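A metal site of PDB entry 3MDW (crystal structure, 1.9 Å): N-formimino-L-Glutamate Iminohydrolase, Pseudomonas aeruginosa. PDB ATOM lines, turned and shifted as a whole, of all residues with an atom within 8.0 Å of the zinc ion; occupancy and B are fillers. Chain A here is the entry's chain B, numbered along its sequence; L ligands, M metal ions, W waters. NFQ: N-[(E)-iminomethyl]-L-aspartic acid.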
ATOM      1  N   HIS A  56       9.018  -4.893  16.728  1.00  0.00           N
ATOM      2  CA  HIS A  56       7.794  -5.044  15.950  1.00  0.00           C
ATOM      3  C   HIS A  56       7.010  -6.294  16.337  1.00  0.00           C
ATOM      4  O   HIS A  56       7.478  -7.416  16.120  1.00  0.00           O
ATOM      5  CB  HIS A  56       8.125  -5.041  14.450  1.00  0.00           C
ATOM      6  CG  HIS A  56       6.921  -5.003  13.573  1.00  0.00           C
ATOM      7  ND1 HIS A  56       6.148  -3.871  13.420  1.00  0.00           N
ATOM      8  CD2 HIS A  56       6.327  -5.964  12.822  1.00  0.00           C
ATOM      9  CE1 HIS A  56       5.154  -4.126  12.586  1.00  0.00           C
ATOM     10  NE2 HIS A  56       5.237  -5.392  12.218  1.00  0.00           N
ATOM     11  N   SER A  57       5.808  -6.085  16.891  1.00  0.00           N
ATOM     12  CA  SER A  57       4.912  -7.156  17.346  1.00  0.00           C
ATOM     13  C   SER A  57       3.438  -6.877  17.015  1.00  0.00           C
ATOM     14  O   SER A  57       2.974  -5.745  17.164  1.00  0.00           O
ATOM     15  CB  SER A  57       5.024  -7.318  18.862  1.00  0.00           C
ATOM     16  OG  SER A  57       3.980  -8.128  19.396  1.00  0.00           O
ATOM     17  N   HIS A  58       2.700  -7.915  16.582  1.00  0.00           N
ATOM     18  CA  HIS A  58       1.225  -7.870  16.639  1.00  0.00           C
ATOM     19  C   HIS A  58       0.749  -9.010  17.520  1.00  0.00           C
ATOM     20  O   HIS A  58       0.535 -10.113  17.030  1.00  0.00           O
ATOM     21  CB  HIS A  58       0.579  -8.029  15.269  1.00  0.00           C
ATOM     22  CG  HIS A  58       1.228  -7.229  14.198  1.00  0.00           C
ATOM     23  ND1 HIS A  58       1.215  -5.847  14.202  1.00  0.00           N
ATOM     24  CD2 HIS A  58       1.887  -7.608  13.089  1.00  0.00           C
ATOM     25  CE1 HIS A  58       1.861  -5.410  13.138  1.00  0.00           C
ATOM     26  NE2 HIS A  58       2.280  -6.457  12.444  1.00  0.00           N
ATOM     27  N   GLN A  61      -1.553 -12.284  16.877  1.00  0.00           N
ATOM     28  CA  GLN A  61      -1.138 -13.258  15.868  1.00  0.00           C
ATOM     29  C   GLN A  61      -0.441 -14.500  16.439  1.00  0.00           C
ATOM     30  O   GLN A  61      -0.446 -15.561  15.825  1.00  0.00           O
ATOM     31  CB  GLN A  61      -0.304 -12.599  14.739  1.00  0.00           C
ATOM     32  CG  GLN A  61      -1.093 -11.522  13.987  1.00  0.00           C
ATOM     33  CD  GLN A  61      -0.335 -10.906  12.805  1.00  0.00           C
ATOM     34  OE1 GLN A  61       0.783 -11.318  12.486  1.00  0.00           O
ATOM     35  NE2 GLN A  61      -0.944  -9.906  12.165  1.00  0.00           N
ATOM     36  N   PHE A  78       0.994 -14.348   0.435  1.00  0.00           N
ATOM     37  CA  PHE A  78       0.917 -13.412   1.540  1.00  0.00           C
ATOM     38  C   PHE A  78      -0.524 -12.928   1.766  1.00  0.00           C
ATOM     39  O   PHE A  78      -0.962 -12.709   2.902  1.00  0.00           O
ATOM     40  CB  PHE A  78       1.844 -12.226   1.239  1.00  0.00           C
ATOM     41  CG  PHE A  78       1.738 -11.099   2.207  1.00  0.00           C
ATOM     42  CD1 PHE A  78       2.675 -10.944   3.217  1.00  0.00           C
ATOM     43  CD2 PHE A  78       0.710 -10.168   2.101  1.00  0.00           C
ATOM     44  CE1 PHE A  78       2.592  -9.893   4.112  1.00  0.00           C
ATOM     45  CE2 PHE A  78       0.622  -9.106   2.990  1.00  0.00           C
ATOM     46  CZ  PHE A  78       1.555  -8.974   4.009  1.00  0.00           C
ATOM     47  N   TRP A  81      -2.913 -15.663   3.242  1.00  0.00           N
ATOM     48  CA  TRP A  81      -2.611 -15.673   4.669  1.00  0.00           C
ATOM     49  C   TRP A  81      -3.303 -14.492   5.367  1.00  0.00           C
ATOM     50  O   TRP A  81      -3.932 -14.658   6.413  1.00  0.00           O
ATOM     51  CB  TRP A  81      -1.102 -15.619   4.919  1.00  0.00           C
ATOM     52  CG  TRP A  81      -0.743 -15.348   6.348  1.00  0.00           C
ATOM     53  CD1 TRP A  81      -0.541 -16.270   7.328  1.00  0.00           C
ATOM     54  CD2 TRP A  81      -0.526 -14.065   6.941  1.00  0.00           C
ATOM     55  NE1 TRP A  81      -0.211 -15.635   8.503  1.00  0.00           N
ATOM     56  CE2 TRP A  81      -0.199 -14.279   8.294  1.00  0.00           C
ATOM     57  CE3 TRP A  81      -0.561 -12.749   6.451  1.00  0.00           C
ATOM     58  CZ2 TRP A  81       0.073 -13.239   9.172  1.00  0.00           C
ATOM     59  CZ3 TRP A  81      -0.295 -11.715   7.323  1.00  0.00           C
ATOM     60  CH2 TRP A  81       0.017 -11.963   8.673  1.00  0.00           C
ATOM     61  N   PHE A 119       2.782  -3.033  17.717  1.00  0.00           N
ATOM     62  CA  PHE A 119       2.285  -2.342  16.538  1.00  0.00           C
ATOM     63  C   PHE A 119       0.788  -2.673  16.474  1.00  0.00           C
ATOM     64  O   PHE A 119       0.370  -3.635  15.836  1.00  0.00           O
ATOM     65  CB  PHE A 119       3.052  -2.860  15.325  1.00  0.00           C
ATOM     66  CG  PHE A 119       2.897  -2.041  14.059  1.00  0.00           C
ATOM     67  CD1 PHE A 119       1.739  -2.132  13.294  1.00  0.00           C
ATOM     68  CD2 PHE A 119       3.933  -1.254  13.608  1.00  0.00           C
ATOM     69  CE1 PHE A 119       1.611  -1.435  12.100  1.00  0.00           C
ATOM     70  CE2 PHE A 119       3.825  -0.552  12.424  1.00  0.00           C
ATOM     71  CZ  PHE A 119       2.657  -0.642  11.668  1.00  0.00           C
ATOM     72  N   TYR A 121      -3.134  -2.444  15.962  1.00  0.00           N
ATOM     73  CA  TYR A 121      -4.153  -1.912  15.074  1.00  0.00           C
ATOM     74  C   TYR A 121      -5.568  -2.458  15.309  1.00  0.00           C
ATOM     75  O   TYR A 121      -6.482  -2.133  14.543  1.00  0.00           O
ATOM     76  CB  TYR A 121      -3.756  -2.080  13.598  1.00  0.00           C
ATOM     77  CG  TYR A 121      -3.390  -3.504  13.188  1.00  0.00           C
ATOM     78  CD1 TYR A 121      -4.361  -4.472  12.989  1.00  0.00           C
ATOM     79  CD2 TYR A 121      -2.067  -3.855  12.958  1.00  0.00           C
ATOM     80  CE1 TYR A 121      -4.025  -5.762  12.602  1.00  0.00           C
ATOM     81  CE2 TYR A 121      -1.713  -5.134  12.560  1.00  0.00           C
ATOM     82  CZ  TYR A 121      -2.705  -6.090  12.389  1.00  0.00           C
ATOM     83  OH  TYR A 121      -2.372  -7.362  11.988  1.00  0.00           O
ATOM     84  N   HIS A 206      -0.134   2.343   9.406  1.00  0.00           N
ATOM     85  CA  HIS A 206      -0.053   0.921   9.104  1.00  0.00           C
ATOM     86  C   HIS A 206       0.832   0.629   7.896  1.00  0.00           C
ATOM     87  O   HIS A 206       1.649  -0.304   7.914  1.00  0.00           O
ATOM     88  CB  HIS A 206      -1.424   0.323   8.850  1.00  0.00           C
ATOM     89  CG  HIS A 206      -1.367  -1.127   8.495  1.00  0.00           C
ATOM     90  ND1 HIS A 206      -1.246  -1.564   7.190  1.00  0.00           N
ATOM     91  CD2 HIS A 206      -1.346  -2.232   9.268  1.00  0.00           C
ATOM     92  CE1 HIS A 206      -1.187  -2.890   7.188  1.00  0.00           C
ATOM     93  NE2 HIS A 206      -1.249  -3.318   8.428  1.00  0.00           N
ATOM     94  N   ILE A 231       6.142   2.368  10.441  1.00  0.00           N
ATOM     95  CA  ILE A 231       5.285   2.082   9.297  1.00  0.00           C
ATOM     96  C   ILE A 231       5.740   0.779   8.621  1.00  0.00           C
ATOM     97  O   ILE A 231       6.955   0.543   8.518  1.00  0.00           O
ATOM     98  CB  ILE A 231       5.316   3.269   8.283  1.00  0.00           C
ATOM     99  CG1 ILE A 231       4.290   3.077   7.157  1.00  0.00           C
ATOM    100  CG2 ILE A 231       6.732   3.455   7.731  1.00  0.00           C
ATOM    101  CD1 ILE A 231       4.183   4.289   6.196  1.00  0.00           C
ATOM    102  N   HIS A 232       4.809  -0.089   8.228  1.00  0.00           N
ATOM    103  CA  HIS A 232       5.164  -1.238   7.368  1.00  0.00           C
ATOM    104  C   HIS A 232       5.449  -0.654   6.001  1.00  0.00           C
ATOM    105  O   HIS A 232       4.656   0.136   5.498  1.00  0.00           O
ATOM    106  CB  HIS A 232       3.990  -2.186   7.137  1.00  0.00           C
ATOM    107  CG  HIS A 232       3.575  -2.997   8.319  1.00  0.00           C
ATOM    108  ND1 HIS A 232       2.327  -2.883   8.892  1.00  0.00           N
ATOM    109  CD2 HIS A 232       4.199  -4.003   8.984  1.00  0.00           C
ATOM    110  CE1 HIS A 232       2.222  -3.750   9.885  1.00  0.00           C
ATOM    111  NE2 HIS A 232       3.342  -4.442   9.960  1.00  0.00           N
ATOM    112  N   GLU A 235       7.122  -4.475   1.971  1.00  0.00           N
ATOM    113  CA  GLU A 235       7.260  -5.866   2.387  1.00  0.00           C
ATOM    114  C   GLU A 235       7.088  -6.843   1.219  1.00  0.00           C
ATOM    115  O   GLU A 235       7.819  -7.837   1.106  1.00  0.00           O
ATOM    116  CB  GLU A 235       6.262  -6.217   3.498  1.00  0.00           C
ATOM    117  CG  GLU A 235       6.509  -7.582   4.090  1.00  0.00           C
ATOM    118  CD  GLU A 235       5.457  -7.972   5.120  1.00  0.00           C
ATOM    119  OE1 GLU A 235       4.559  -7.149   5.366  1.00  0.00           O
ATOM    120  OE2 GLU A 235       5.547  -9.082   5.683  1.00  0.00           O
ATOM    121  N   VAL A 268       9.444  -0.800   8.870  1.00  0.00           N
ATOM    122  CA  VAL A 268       9.340  -2.227   9.140  1.00  0.00           C
ATOM    123  C   VAL A 268       9.350  -2.999   7.841  1.00  0.00           C
ATOM    124  O   VAL A 268       8.599  -2.682   6.929  1.00  0.00           O
ATOM    125  CB  VAL A 268       8.074  -2.556   9.937  1.00  0.00           C
ATOM    126  CG1 VAL A 268       8.045  -4.038  10.303  1.00  0.00           C
ATOM    127  CG2 VAL A 268       8.004  -1.689  11.172  1.00  0.00           C
ATOM    128  N   HIS A 269      10.207  -4.027   7.804  1.00  0.00           N
ATOM    129  CA  HIS A 269      10.492  -4.881   6.641  1.00  0.00           C
ATOM    130  C   HIS A 269      11.420  -4.196   5.632  1.00  0.00           C
ATOM    131  O   HIS A 269      12.580  -4.586   5.492  1.00  0.00           O
ATOM    132  CB  HIS A 269       9.236  -5.383   5.959  1.00  0.00           C
ATOM    133  CG  HIS A 269       8.267  -6.054   6.877  1.00  0.00           C
ATOM    134  ND1 HIS A 269       8.608  -7.163   7.627  1.00  0.00           N
ATOM    135  CD2 HIS A 269       6.976  -5.779   7.162  1.00  0.00           C
ATOM    136  CE1 HIS A 269       7.558  -7.537   8.341  1.00  0.00           C
ATOM    137  NE2 HIS A 269       6.552  -6.718   8.074  1.00  0.00           N
ATOM    138  N   CYS A 291      12.228  -8.483  10.388  1.00  0.00           N
ATOM    139  CA  CYS A 291      11.464  -9.541  11.041  1.00  0.00           C
ATOM    140  C   CYS A 291      11.714 -10.824  10.282  1.00  0.00           C
ATOM    141  O   CYS A 291      10.911 -11.232   9.446  1.00  0.00           O
ATOM    142  CB  CYS A 291       9.973  -9.184  10.987  1.00  0.00           C
ATOM    143  SG  CYS A 291       9.606  -7.584  11.773  1.00  0.00           S
ATOM    144  N   THR A 294       9.331 -14.107  10.315  1.00  0.00           N
ATOM    145  CA  THR A 294       8.051 -13.810   9.688  1.00  0.00           C
ATOM    146  C   THR A 294       8.204 -13.585   8.179  1.00  0.00           C
ATOM    147  O   THR A 294       7.430 -14.115   7.378  1.00  0.00           O
ATOM    148  CB  THR A 294       7.332 -12.628  10.378  1.00  0.00           C
ATOM    149  OG1 THR A 294       6.830 -13.058  11.652  1.00  0.00           O
ATOM    150  CG2 THR A 294       6.187 -12.119   9.524  1.00  0.00           C
ATOM    151  N   LEU A 298       6.323 -15.771   5.444  1.00  0.00           N
ATOM    152  CA  LEU A 298       5.353 -15.184   4.521  1.00  0.00           C
ATOM    153  C   LEU A 298       5.885 -15.120   3.097  1.00  0.00           C
ATOM    154  O   LEU A 298       5.182 -14.649   2.193  1.00  0.00           O
ATOM    155  CB  LEU A 298       4.958 -13.782   4.983  1.00  0.00           C
ATOM    156  CG  LEU A 298       4.259 -13.717   6.336  1.00  0.00           C
ATOM    157  CD1 LEU A 298       3.897 -12.259   6.658  1.00  0.00           C
ATOM    158  CD2 LEU A 298       3.015 -14.613   6.360  1.00  0.00           C
ATOM    159  N   SER A 319       9.657  -9.851  16.126  1.00  0.00           N
ATOM    160  CA  SER A 319       9.079 -11.172  15.904  1.00  0.00           C
ATOM    161  C   SER A 319       7.763 -11.111  15.125  1.00  0.00           C
ATOM    162  O   SER A 319       7.270 -12.150  14.675  1.00  0.00           O
ATOM    163  CB  SER A 319       8.920 -11.930  17.236  1.00  0.00           C
ATOM    164  OG  SER A 319       8.148 -11.189  18.165  1.00  0.00           O
ATOM    165  N   ASP A 320       7.203  -9.913  14.978  1.00  0.00           N
ATOM    166  CA  ASP A 320       6.096  -9.655  14.047  1.00  0.00           C
ATOM    167  C   ASP A 320       4.860 -10.569  14.200  1.00  0.00           C
ATOM    168  O   ASP A 320       4.024 -10.327  15.072  1.00  0.00           O
ATOM    169  CB  ASP A 320       6.623  -9.672  12.602  1.00  0.00           C
ATOM    170  CG  ASP A 320       5.629  -9.102  11.596  1.00  0.00           C
ATOM    171  OD1 ASP A 320       4.580  -8.589  12.007  1.00  0.00           O
ATOM    172  OD2 ASP A 320       5.920  -9.164  10.378  1.00  0.00           O
ATOM    173  N   SER A 321       4.729 -11.591  13.350  1.00  0.00           N
ATOM    174  CA  SER A 321       3.615 -12.563  13.448  1.00  0.00           C
ATOM    175  C   SER A 321       3.827 -13.570  14.572  1.00  0.00           C
ATOM    176  O   SER A 321       2.917 -14.335  14.937  1.00  0.00           O
ATOM    177  CB  SER A 321       3.399 -13.296  12.124  1.00  0.00           C
ATOM    178  OG  SER A 321       4.391 -14.291  11.910  1.00  0.00           O
HETATM  179  C   NFQ L   1      -0.298  -6.736   9.282  1.00  0.00           C
HETATM  180  N   NFQ L   1       1.497  -8.121   8.271  1.00  0.00           N
HETATM  181  O1  NFQ L   1      -1.038  -5.743   9.317  1.00  0.00           O
HETATM  182  O2  NFQ L   1      -0.417  -7.626  10.154  1.00  0.00           O
HETATM  183  CA  NFQ L   1       0.571  -6.999   8.027  1.00  0.00           C
HETATM  184  CB  NFQ L   1      -0.344  -7.220   6.812  1.00  0.00           C
HETATM  185  CF  NFQ L   1       2.564  -8.454   7.313  1.00  0.00           C
HETATM  186  NF  NFQ L   1       3.468  -9.250   7.667  1.00  0.00           N
HETATM  187  CG  NFQ L   1      -0.407  -5.975   5.912  1.00  0.00           C
HETATM  188  OD1 NFQ L   1       0.625  -5.283   5.769  1.00  0.00           O
HETATM  189  OD2 NFQ L   1      -1.525  -5.614   5.490  1.00  0.00           O
HETATM  190 ZN    ZN M   1       3.772  -6.316  11.026  1.00  0.00          ZN
HETATM  191  O   HOH W   1       4.211  -7.492   9.415  1.00  0.00           O
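The nearest printed residue that does not touch the zinc ion is His 269 (4.1 Å).
Water W1 lies within hydrogen-bond range of the side-chain carboxylate (OD2) of Asp 320 (2.6 Å), a nitrogen (NF) of the ligand (2.6 Å) and a ring nitrogen (NE2) of His 269 (2.8 Å).
The zinc ion is bound by water W1 (2.0 Å), a ring nitrogen (NE2) of His 58 (2.1 Å), a ring nitrogen (NE2) of His 56 (2.1 Å) and a ring nitrogen (NE2) of His 232 (2.2 Å).
Slightly farther from the zinc ion lies the side-chain carboxylate (OD1) of Asp 320 (2.6 Å).
The backbone NH of Ser 319 lies within hydrogen-bond range of the backbone carbonyl oxygen of His 56 (3.3 Å).
A ring nitrogen (NE2) of His 269 lies close to the side-chain carboxylate of Asp 320 (3.4 Å).
N of His 58 lies within hydrogen-bond range of O of Asp 320, 3.1 Å away.
The backbone carbonyl oxygen (O) of His 56 lies within hydrogen-bond range of the backbone NH (N) of Asp 320 (2.8 Å).
O of His 206 is in hydrogen-bond range of ND1 of His 232 (2.8 Å).
A ring nitrogen (ND1) of His 58 is in hydrogen-bond range of the backbone carbonyl oxygen (O) of Phe 119, at 2.9 Å.
A nitrogen (NF) of the ligand lies within salt-bridge range of the side-chain carboxylate of Glu 235 (2.9 Å).
NE2 of His 206 is in hydrogen-bond range of O1 of the ligand, at 2.6 Å.
OH of Tyr 121 sits at hydrogen-bond distance from O2 of the ligand (2.7 Å).
The side-chain amide nitrogen (NE2) of Gln 61 lies within hydrogen-bond range of an oxygen (O2) of the ligand (3.1 Å).
The side-chain carboxylate (OD2) of Asp 320 is in salt-bridge range of a nitrogen (NF) of the ligand (3.7 Å).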
